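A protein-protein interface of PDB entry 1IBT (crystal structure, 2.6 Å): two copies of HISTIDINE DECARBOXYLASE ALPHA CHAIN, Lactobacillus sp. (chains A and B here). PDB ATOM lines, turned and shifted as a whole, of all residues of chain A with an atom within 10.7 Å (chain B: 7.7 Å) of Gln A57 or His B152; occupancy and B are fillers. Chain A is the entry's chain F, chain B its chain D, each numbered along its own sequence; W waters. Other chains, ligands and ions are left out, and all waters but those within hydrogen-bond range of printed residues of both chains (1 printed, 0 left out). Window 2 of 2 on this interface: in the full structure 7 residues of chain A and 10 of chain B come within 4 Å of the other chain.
The backbone carbonyl oxygen (O) of His B152 lies within hydrogen-bond range of the side-chain amino group (NZ) of Lys B109 (3.1 Å). The side-chain amide nitrogen (NE2) of Gln B149 lies within hydrogen-bond range of the side-chain carboxylate (OD2) of Asp B150, at 3.2 Å. O of Gln B149 lies within hydrogen-bond range of ND1 of His B152. The side-chain hydroxyl of Thr A55 lies close to the backbone NH of Gln A57. OE1 of Glu A56 lies close to OE1 of Gln A57, at 3.1 Å. The side-chain carboxylate (OE2) of Glu A56 is in salt-bridge range of the guanidinium group (NH1) of Arg A59 (2.8 Å).
Hydrophobic or aromatic side chains of chain A within 4 Å of the printed part of chain B: Pro A65. Printed residues of chain B that touch a printed residue of chain A: Lys B109, Asp B150, Ala B151 and His B152. Among the printed residues, no Asp or Glu carboxylate lies within 4 Å of a Lys or Arg side-chain nitrogen of the other chain.
O of Ala B151 sits at hydrogen-bond distance from NH2 of Arg A59. OE1 of Glu A56 sits at hydrogen-bond distance from NE2 of His B152 (2.6 Å). The side-chain amide oxygen (OE1) of Gln A57 lies within hydrogen-bond range of a ring nitrogen (NE2) of His B152 (3.2 Å). The side-chain carboxylate (OE2) of Glu A56 sits close to the backbone carbonyl oxygen (O) of Ala B151.
Water W1 bridges the backbone carbonyl oxygen (O) of Lys B109 (2.5 Å) and the side-chain hydroxyl (OH) of Tyr A62 (2.6 Å).
Printed residues of chain B within 4 Å of Glu A56: Asp B150, Ala B151 and His B152. Gln A57 touches just one residue of chain B: His B152. Of the printed residues of chain B, Arg A59 touches Ala B151 (2.9 Å). Of the printed residues of chain B, Pro A65 touches Lys B109 (3.5 Å). Lys A219 touches none of the printed residues of chain B. Leu A227 touches none of the printed residues of chain B. Of the printed residues of chain A, Lys B109 touches Pro A65. No residue of chain A comes within 4 Å of Gly B148. Of the printed residues of chain A, Asp B150 touches Glu A56 (3.5 Å). Ala B151 touches two residues of chain A. His B152 touches two residues of chain A. Ala B153 touches none of the printed residues of chain A. No residue of chain A comes within 4 Å of Ser B154. The nearest printed residue of chain B that does not touch Arg A59 is Asp B110 (4.5 Å).
No position is printed for both chains. Of the 6 pairs that touch across the chains among the printed residues, none has its exchanged pair printed and touching as well.
Asp B150 touches Glu A56 (O to CG, 3.5 Å). Lys B109 touches Pro A65 (O to CG, 3.5 Å).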
ATOM      1  N   VAL A  50      16.734  21.602   2.822  1.00  0.00           N
ATOM      2  CA  VAL A  50      16.220  22.721   3.611  1.00  0.00           C
ATOM      3  C   VAL A  50      14.719  22.533   3.761  1.00  0.00           C
ATOM      4  O   VAL A  50      14.188  22.772   4.849  1.00  0.00           O
ATOM      5  CB  VAL A  50      16.550  24.072   2.913  1.00  0.00           C
ATOM      6  CG1 VAL A  50      16.250  25.225   3.857  1.00  0.00           C
ATOM      7  CG2 VAL A  50      18.022  24.098   2.510  1.00  0.00           C
ATOM      8  N   PHE A  53      14.624  19.487   6.698  1.00  0.00           N
ATOM      9  CA  PHE A  53      14.955  19.854   8.068  1.00  0.00           C
ATOM     10  C   PHE A  53      14.343  21.152   8.484  1.00  0.00           C
ATOM     11  O   PHE A  53      13.954  21.306   9.640  1.00  0.00           O
ATOM     12  CB  PHE A  53      16.437  20.034   8.326  1.00  0.00           C
ATOM     13  CG  PHE A  53      17.296  18.786   8.295  1.00  0.00           C
ATOM     14  CD1 PHE A  53      18.671  18.929   8.433  1.00  0.00           C
ATOM     15  CD2 PHE A  53      16.730  17.511   8.133  1.00  0.00           C
ATOM     16  CE1 PHE A  53      19.474  17.799   8.409  1.00  0.00           C
ATOM     17  CE2 PHE A  53      17.546  16.389   8.110  1.00  0.00           C
ATOM     18  CZ  PHE A  53      18.924  16.532   8.249  1.00  0.00           C
ATOM     19  N   GLY A  54      14.238  22.083   7.548  1.00  0.00           N
ATOM     20  CA  GLY A  54      13.723  23.388   7.866  1.00  0.00           C
ATOM     21  C   GLY A  54      14.848  24.258   8.361  1.00  0.00           C
ATOM     22  O   GLY A  54      15.995  23.837   8.338  1.00  0.00           O
ATOM     23  N   THR A  55      14.539  25.467   8.831  1.00  0.00           N
ATOM     24  CA  THR A  55      15.544  26.427   9.227  1.00  0.00           C
ATOM     25  C   THR A  55      15.402  26.694  10.701  1.00  0.00           C
ATOM     26  O   THR A  55      14.364  26.365  11.270  1.00  0.00           O
ATOM     27  CB  THR A  55      15.356  27.708   8.446  1.00  0.00           C
ATOM     28  OG1 THR A  55      14.270  28.369   9.054  1.00  0.00           O
ATOM     29  CG2 THR A  55      15.115  27.468   6.968  1.00  0.00           C
ATOM     30  N   GLU A  56      16.354  27.401  11.321  1.00  0.00           N
ATOM     31  CA  GLU A  56      16.284  27.721  12.748  1.00  0.00           C
ATOM     32  C   GLU A  56      14.935  28.314  13.125  1.00  0.00           C
ATOM     33  O   GLU A  56      14.263  27.931  14.087  1.00  0.00           O
ATOM     34  CB  GLU A  56      17.420  28.666  13.019  1.00  0.00           C
ATOM     35  CG  GLU A  56      17.955  28.692  14.441  1.00  0.00           C
ATOM     36  CD  GLU A  56      17.131  29.441  15.453  1.00  0.00           C
ATOM     37  OE1 GLU A  56      16.442  30.379  15.074  1.00  0.00           O
ATOM     38  OE2 GLU A  56      17.153  29.062  16.627  1.00  0.00           O
ATOM     39  N   GLN A  57      14.492  29.104  12.158  1.00  0.00           N
ATOM     40  CA  GLN A  57      13.255  29.837  12.254  1.00  0.00           C
ATOM     41  C   GLN A  57      11.998  29.094  11.874  1.00  0.00           C
ATOM     42  O   GLN A  57      10.938  29.478  12.326  1.00  0.00           O
ATOM     43  CB  GLN A  57      13.407  31.101  11.397  1.00  0.00           C
ATOM     44  CG  GLN A  57      14.186  32.144  12.190  1.00  0.00           C
ATOM     45  CD  GLN A  57      13.501  32.522  13.504  1.00  0.00           C
ATOM     46  OE1 GLN A  57      13.867  32.087  14.600  1.00  0.00           O
ATOM     47  NE2 GLN A  57      12.484  33.368  13.446  1.00  0.00           N
ATOM     48  N   ASP A  58      12.106  28.078  11.039  1.00  0.00           N
ATOM     49  CA  ASP A  58      10.995  27.293  10.526  1.00  0.00           C
ATOM     50  C   ASP A  58      11.539  25.881  10.723  1.00  0.00           C
ATOM     51  O   ASP A  58      11.984  25.204   9.789  1.00  0.00           O
ATOM     52  CB  ASP A  58      10.800  27.539   9.046  1.00  0.00           C
ATOM     53  CG  ASP A  58       9.366  27.590   8.607  1.00  0.00           C
ATOM     54  OD1 ASP A  58       8.870  26.667   7.953  1.00  0.00           O
ATOM     55  OD2 ASP A  58       8.704  28.604   8.835  1.00  0.00           O
ATOM     56  N   ARG A  59      11.663  25.466  11.977  1.00  0.00           N
ATOM     57  CA  ARG A  59      12.198  24.145  12.303  1.00  0.00           C
ATOM     58  C   ARG A  59      11.252  23.023  11.885  1.00  0.00           C
ATOM     59  O   ARG A  59      10.102  23.006  12.327  1.00  0.00           O
ATOM     60  CB  ARG A  59      12.469  24.130  13.807  1.00  0.00           C
ATOM     61  CG  ARG A  59      13.817  24.663  14.281  1.00  0.00           C
ATOM     62  CD  ARG A  59      13.610  24.836  15.763  1.00  0.00           C
ATOM     63  NE  ARG A  59      14.761  24.782  16.684  1.00  0.00           N
ATOM     64  CZ  ARG A  59      15.524  25.843  16.994  1.00  0.00           C
ATOM     65  NH1 ARG A  59      15.291  27.031  16.433  1.00  0.00           N
ATOM     66  NH2 ARG A  59      16.429  25.752  17.975  1.00  0.00           N
ATOM     67  N   ARG A  60      11.666  22.120  11.006  1.00  0.00           N
ATOM     68  CA  ARG A  60      10.831  21.010  10.579  1.00  0.00           C
ATOM     69  C   ARG A  60      11.369  19.654  11.053  1.00  0.00           C
ATOM     70  O   ARG A  60      11.354  19.391  12.261  1.00  0.00           O
ATOM     71  CB  ARG A  60      10.694  20.967   9.066  1.00  0.00           C
ATOM     72  CG  ARG A  60       9.872  22.122   8.564  1.00  0.00           C
ATOM     73  CD  ARG A  60       9.858  22.129   7.067  1.00  0.00           C
ATOM     74  NE  ARG A  60       9.196  23.346   6.645  1.00  0.00           N
ATOM     75  CZ  ARG A  60       9.065  23.686   5.362  1.00  0.00           C
ATOM     76  NH1 ARG A  60       8.440  24.806   5.145  1.00  0.00           N
ATOM     77  NH2 ARG A  60       9.553  22.996   4.327  1.00  0.00           N
ATOM     78  N   HIS A  61      11.860  18.724  10.232  1.00  0.00           N
ATOM     79  CA  HIS A  61      12.277  17.442  10.737  1.00  0.00           C
ATOM     80  C   HIS A  61      13.789  17.399  10.848  1.00  0.00           C
ATOM     81  O   HIS A  61      14.519  16.646  10.202  1.00  0.00           O
ATOM     82  CB  HIS A  61      11.703  16.376   9.796  1.00  0.00           C
ATOM     83  CG  HIS A  61      10.185  16.458   9.856  1.00  0.00           C
ATOM     84  ND1 HIS A  61       9.384  16.275  10.899  1.00  0.00           N
ATOM     85  CD2 HIS A  61       9.387  16.827   8.807  1.00  0.00           C
ATOM     86  CE1 HIS A  61       8.154  16.525  10.541  1.00  0.00           C
ATOM     87  NE2 HIS A  61       8.170  16.858   9.282  1.00  0.00           N
ATOM     88  N   TYR A  62      14.261  18.267  11.722  1.00  0.00           N
ATOM     89  CA  TYR A  62      15.684  18.423  11.938  1.00  0.00           C
ATOM     90  C   TYR A  62      16.196  17.372  12.898  1.00  0.00           C
ATOM     91  O   TYR A  62      15.380  16.655  13.464  1.00  0.00           O
ATOM     92  CB  TYR A  62      15.939  19.807  12.467  1.00  0.00           C
ATOM     93  CG  TYR A  62      15.337  20.129  13.791  1.00  0.00           C
ATOM     94  CD1 TYR A  62      14.067  20.645  13.865  1.00  0.00           C
ATOM     95  CD2 TYR A  62      16.074  19.949  14.934  1.00  0.00           C
ATOM     96  CE1 TYR A  62      13.532  20.987  15.099  1.00  0.00           C
ATOM     97  CE2 TYR A  62      15.548  20.293  16.176  1.00  0.00           C
ATOM     98  CZ  TYR A  62      14.275  20.809  16.237  1.00  0.00           C
ATOM     99  OH  TYR A  62      13.727  21.146  17.431  1.00  0.00           O
ATOM    100  N   PRO A  65      17.640  17.063  19.453  1.00  0.00           N
ATOM    101  CA  PRO A  65      18.565  17.685  20.375  1.00  0.00           C
ATOM    102  C   PRO A  65      19.527  16.711  21.027  1.00  0.00           C
ATOM    103  O   PRO A  65      19.049  15.871  21.782  1.00  0.00           O
ATOM    104  CB  PRO A  65      17.654  18.380  21.350  1.00  0.00           C
ATOM    105  CG  PRO A  65      16.519  18.826  20.498  1.00  0.00           C
ATOM    106  CD  PRO A  65      16.313  17.581  19.663  1.00  0.00           C
ATOM    107  N   LYS A 219       4.812  25.236   3.263  1.00  0.00           N
ATOM    108  CA  LYS A 219       5.225  26.281   2.305  1.00  0.00           C
ATOM    109  C   LYS A 219       6.637  25.978   1.809  1.00  0.00           C
ATOM    110  O   LYS A 219       7.486  25.573   2.617  1.00  0.00           O
ATOM    111  CB  LYS A 219       5.186  27.653   3.008  1.00  0.00           C
ATOM    112  CG  LYS A 219       5.728  27.619   4.475  1.00  0.00           C
ATOM    113  CD  LYS A 219       5.220  28.848   5.288  1.00  0.00           C
ATOM    114  CE  LYS A 219       5.298  28.682   6.843  1.00  0.00           C
ATOM    115  NZ  LYS A 219       6.646  28.423   7.361  1.00  0.00           N
ATOM    116  N   LEU A 221      10.232  26.549   0.940  1.00  0.00           N
ATOM    117  CA  LEU A 221      11.190  27.502   1.419  1.00  0.00           C
ATOM    118  C   LEU A 221      12.165  27.869   0.324  1.00  0.00           C
ATOM    119  O   LEU A 221      13.019  28.725   0.542  1.00  0.00           O
ATOM    120  CB  LEU A 221      11.898  26.906   2.611  1.00  0.00           C
ATOM    121  CG  LEU A 221      11.083  26.769   3.876  1.00  0.00           C
ATOM    122  CD1 LEU A 221      11.952  26.127   4.920  1.00  0.00           C
ATOM    123  CD2 LEU A 221      10.605  28.111   4.385  1.00  0.00           C
ATOM    124  N   LEU A 227      16.627  30.632  -1.623  1.00  0.00           N
ATOM    125  CA  LEU A 227      17.646  30.041  -0.771  1.00  0.00           C
ATOM    126  C   LEU A 227      19.052  30.298  -1.313  1.00  0.00           C
ATOM    127  O   LEU A 227      19.381  29.940  -2.463  1.00  0.00           O
ATOM    128  CB  LEU A 227      17.319  28.540  -0.675  1.00  0.00           C
ATOM    129  CG  LEU A 227      16.888  27.874   0.652  1.00  0.00           C
ATOM    130  CD1 LEU A 227      16.172  28.786   1.651  1.00  0.00           C
ATOM    131  CD2 LEU A 227      15.954  26.783   0.231  1.00  0.00           C
ATOM    132  N   GLN B  31      22.167  36.409  28.536  1.00  0.00           N
ATOM    133  CA  GLN B  31      22.061  35.717  27.270  1.00  0.00           C
ATOM    134  C   GLN B  31      20.920  36.329  26.509  1.00  0.00           C
ATOM    135  O   GLN B  31      20.211  37.172  27.056  1.00  0.00           O
ATOM    136  CB  GLN B  31      21.871  34.227  27.498  1.00  0.00           C
ATOM    137  CG  GLN B  31      20.844  33.689  28.499  1.00  0.00           C
ATOM    138  CD  GLN B  31      20.995  32.202  28.845  1.00  0.00           C
ATOM    139  OE1 GLN B  31      21.462  31.343  28.076  1.00  0.00           O
ATOM    140  NE2 GLN B  31      20.569  31.865  30.046  1.00  0.00           N
ATOM    141  N   TRP B  32      20.708  35.951  25.256  1.00  0.00           N
ATOM    142  CA  TRP B  32      19.816  36.603  24.299  1.00  0.00           C
ATOM    143  C   TRP B  32      18.386  36.959  24.692  1.00  0.00           C
ATOM    144  O   TRP B  32      17.694  37.678  23.965  1.00  0.00           O
ATOM    145  CB  TRP B  32      19.771  35.732  23.042  1.00  0.00           C
ATOM    146  CG  TRP B  32      19.025  34.431  23.338  1.00  0.00           C
ATOM    147  CD1 TRP B  32      19.661  33.326  23.871  1.00  0.00           C
ATOM    148  CD2 TRP B  32      17.664  34.215  23.150  1.00  0.00           C
ATOM    149  NE1 TRP B  32      18.720  32.413  24.025  1.00  0.00           N
ATOM    150  CE2 TRP B  32      17.516  32.879  23.609  1.00  0.00           C
ATOM    151  CE3 TRP B  32      16.562  34.946  22.664  1.00  0.00           C
ATOM    152  CZ2 TRP B  32      16.257  32.259  23.579  1.00  0.00           C
ATOM    153  CZ3 TRP B  32      15.312  34.316  22.644  1.00  0.00           C
ATOM    154  CH2 TRP B  32      15.160  32.986  23.093  1.00  0.00           C
ATOM    155  N   ASP B  33      17.877  36.349  25.733  1.00  0.00           N
ATOM    156  CA  ASP B  33      16.521  36.581  26.204  1.00  0.00           C
ATOM    157  C   ASP B  33      16.519  37.580  27.370  1.00  0.00           C
ATOM    158  O   ASP B  33      15.511  38.180  27.772  1.00  0.00           O
ATOM    159  CB  ASP B  33      15.948  35.202  26.609  1.00  0.00           C
ATOM    160  CG  ASP B  33      16.730  34.461  27.701  1.00  0.00           C
ATOM    161  OD1 ASP B  33      16.194  33.531  28.311  1.00  0.00           O
ATOM    162  OD2 ASP B  33      17.891  34.801  27.966  1.00  0.00           O
ATOM    163  N   LYS B 105      17.315  25.080  29.600  1.00  0.00           N
ATOM    164  CA  LYS B 105      16.212  25.489  30.451  1.00  0.00           C
ATOM    165  C   LYS B 105      15.031  24.569  30.166  1.00  0.00           C
ATOM    166  O   LYS B 105      14.362  24.101  31.087  1.00  0.00           O
ATOM    167  CB  LYS B 105      15.927  26.938  30.121  1.00  0.00           C
ATOM    168  CG  LYS B 105      14.811  27.749  30.794  1.00  0.00           C
ATOM    169  CD  LYS B 105      14.371  28.777  29.693  1.00  0.00           C
ATOM    170  CE  LYS B 105      13.838  28.108  28.350  1.00  0.00           C
ATOM    171  NZ  LYS B 105      13.969  28.918  27.128  1.00  0.00           N
ATOM    172  N   LYS B 109      12.713  20.975  24.445  1.00  0.00           N
ATOM    173  CA  LYS B 109      12.887  21.663  23.186  1.00  0.00           C
ATOM    174  C   LYS B 109      14.386  21.787  22.825  1.00  0.00           C
ATOM    175  O   LYS B 109      14.784  21.613  21.660  1.00  0.00           O
ATOM    176  CB  LYS B 109      12.147  23.033  23.347  1.00  0.00           C
ATOM    177  CG  LYS B 109      12.347  24.170  22.300  1.00  0.00           C
ATOM    178  CD  LYS B 109      12.068  25.535  22.997  1.00  0.00           C
ATOM    179  CE  LYS B 109      12.666  26.771  22.286  1.00  0.00           C
ATOM    180  NZ  LYS B 109      14.119  26.777  22.389  1.00  0.00           N
ATOM    181  N   ASP B 110      15.226  22.031  23.828  1.00  0.00           N
ATOM    182  CA  ASP B 110      16.617  22.367  23.607  1.00  0.00           C
ATOM    183  C   ASP B 110      17.615  21.413  24.224  1.00  0.00           C
ATOM    184  O   ASP B 110      17.354  20.822  25.265  1.00  0.00           O
ATOM    185  CB  ASP B 110      16.940  23.763  24.184  1.00  0.00           C
ATOM    186  CG  ASP B 110      16.177  24.941  23.619  1.00  0.00           C
ATOM    187  OD1 ASP B 110      16.082  25.079  22.391  1.00  0.00           O
ATOM    188  OD2 ASP B 110      15.631  25.728  24.400  1.00  0.00           O
ATOM    189  N   GLU B 146      26.877  33.292  23.147  1.00  0.00           N
ATOM    190  CA  GLU B 146      26.837  33.502  21.690  1.00  0.00           C
ATOM    191  C   GLU B 146      26.026  32.328  21.164  1.00  0.00           C
ATOM    192  O   GLU B 146      24.868  32.558  20.790  1.00  0.00           O
ATOM    193  CB  GLU B 146      28.208  33.411  20.946  1.00  0.00           C
ATOM    194  CG  GLU B 146      29.436  34.231  21.347  1.00  0.00           C
ATOM    195  CD  GLU B 146      29.431  35.700  20.978  1.00  0.00           C
ATOM    196  OE1 GLU B 146      29.683  36.525  21.861  1.00  0.00           O
ATOM    197  OE2 GLU B 146      29.242  35.977  19.793  1.00  0.00           O
ATOM    198  N   CYS B 147      26.577  31.099  21.344  1.00  0.00           N
ATOM    199  CA  CYS B 147      25.992  29.846  20.866  1.00  0.00           C
ATOM    200  C   CYS B 147      24.530  29.733  21.260  1.00  0.00           C
ATOM    201  O   CYS B 147      23.657  29.505  20.432  1.00  0.00           O
ATOM    202  CB  CYS B 147      26.791  28.662  21.426  1.00  0.00           C
ATOM    203  SG  CYS B 147      28.251  28.066  20.473  1.00  0.00           S
ATOM    204  N   GLY B 148      24.177  30.069  22.494  1.00  0.00           N
ATOM    205  CA  GLY B 148      22.801  30.046  22.980  1.00  0.00           C
ATOM    206  C   GLY B 148      21.838  30.734  22.028  1.00  0.00           C
ATOM    207  O   GLY B 148      20.882  30.121  21.538  1.00  0.00           O
ATOM    208  N   GLN B 149      22.177  31.967  21.643  1.00  0.00           N
ATOM    209  CA  GLN B 149      21.357  32.750  20.728  1.00  0.00           C
ATOM    210  C   GLN B 149      21.336  32.132  19.333  1.00  0.00           C
ATOM    211  O   GLN B 149      20.327  32.310  18.630  1.00  0.00           O
ATOM    212  CB  GLN B 149      21.889  34.221  20.731  1.00  0.00           C
ATOM    213  CG  GLN B 149      21.738  35.221  19.565  1.00  0.00           C
ATOM    214  CD  GLN B 149      22.721  34.888  18.428  1.00  0.00           C
ATOM    215  OE1 GLN B 149      22.404  35.010  17.240  1.00  0.00           O
ATOM    216  NE2 GLN B 149      23.962  34.427  18.689  1.00  0.00           N
ATOM    217  N   ASP B 150      22.368  31.394  18.923  1.00  0.00           N
ATOM    218  CA  ASP B 150      22.406  30.772  17.606  1.00  0.00           C
ATOM    219  C   ASP B 150      21.239  29.852  17.327  1.00  0.00           C
ATOM    220  O   ASP B 150      20.815  29.711  16.177  1.00  0.00           O
ATOM    221  CB  ASP B 150      23.652  29.935  17.418  1.00  0.00           C
ATOM    222  CG  ASP B 150      24.909  30.715  17.179  1.00  0.00           C
ATOM    223  OD1 ASP B 150      25.480  30.490  16.106  1.00  0.00           O
ATOM    224  OD2 ASP B 150      25.272  31.579  17.999  1.00  0.00           O
ATOM    225  N   ALA B 151      20.834  29.191  18.427  1.00  0.00           N
ATOM    226  CA  ALA B 151      19.740  28.240  18.446  1.00  0.00           C
ATOM    227  C   ALA B 151      18.576  28.605  19.376  1.00  0.00           C
ATOM    228  O   ALA B 151      17.632  27.830  19.582  1.00  0.00           O
ATOM    229  CB  ALA B 151      20.296  26.864  18.843  1.00  0.00           C
ATOM    230  N   HIS B 152      18.607  29.800  19.948  1.00  0.00           N
ATOM    231  CA  HIS B 152      17.605  30.345  20.865  1.00  0.00           C
ATOM    232  C   HIS B 152      17.275  29.366  21.989  1.00  0.00           C
ATOM    233  O   HIS B 152      16.149  29.142  22.454  1.00  0.00           O
ATOM    234  CB  HIS B 152      16.316  30.743  20.107  1.00  0.00           C
ATOM    235  CG  HIS B 152      16.529  31.623  18.875  1.00  0.00           C
ATOM    236  ND1 HIS B 152      17.460  32.518  18.522  1.00  0.00           N
ATOM    237  CD2 HIS B 152      15.698  31.482  17.793  1.00  0.00           C
ATOM    238  CE1 HIS B 152      17.219  32.883  17.285  1.00  0.00           C
ATOM    239  NE2 HIS B 152      16.158  32.253  16.855  1.00  0.00           N
ATOM    240  N   ALA B 153      18.403  28.850  22.469  1.00  0.00           N
ATOM    241  CA  ALA B 153      18.477  27.911  23.560  1.00  0.00           C
ATOM    242  C   ALA B 153      18.894  28.622  24.820  1.00  0.00           C
ATOM    243  O   ALA B 153      20.082  28.850  24.988  1.00  0.00           O
ATOM    244  CB  ALA B 153      19.504  26.829  23.231  1.00  0.00           C
ATOM    245  N   SER B 154      18.005  29.103  25.682  1.00  0.00           N
ATOM    246  CA  SER B 154      18.425  29.697  26.947  1.00  0.00           C
ATOM    247  C   SER B 154      18.831  28.564  27.854  1.00  0.00           C
ATOM    248  O   SER B 154      18.173  27.512  27.825  1.00  0.00           O
ATOM    249  CB  SER B 154      17.320  30.425  27.672  1.00  0.00           C
ATOM    250  OG  SER B 154      16.152  30.581  26.858  1.00  0.00           O
ATOM    251  N   PHE B 155      19.875  28.724  28.658  1.00  0.00           N
ATOM    252  CA  PHE B 155      20.305  27.681  29.581  1.00  0.00           C
ATOM    253  C   PHE B 155      19.904  28.095  30.968  1.00  0.00           C
ATOM    254  O   PHE B 155      19.404  29.207  31.117  1.00  0.00           O
ATOM    255  CB  PHE B 155      21.808  27.502  29.513  1.00  0.00           C
ATOM    256  CG  PHE B 155      22.292  27.104  28.123  1.00  0.00           C
ATOM    257  CD1 PHE B 155      22.205  25.787  27.702  1.00  0.00           C
ATOM    258  CD2 PHE B 155      22.822  28.069  27.259  1.00  0.00           C
ATOM    259  CE1 PHE B 155      22.648  25.436  26.422  1.00  0.00           C
ATOM    260  CE2 PHE B 155      23.260  27.707  25.986  1.00  0.00           C
ATOM    261  CZ  PHE B 155      23.178  26.393  25.557  1.00  0.00           C
HETATM  262  O   HOH W   1      15.482  21.574  19.279  1.00  0.00           O
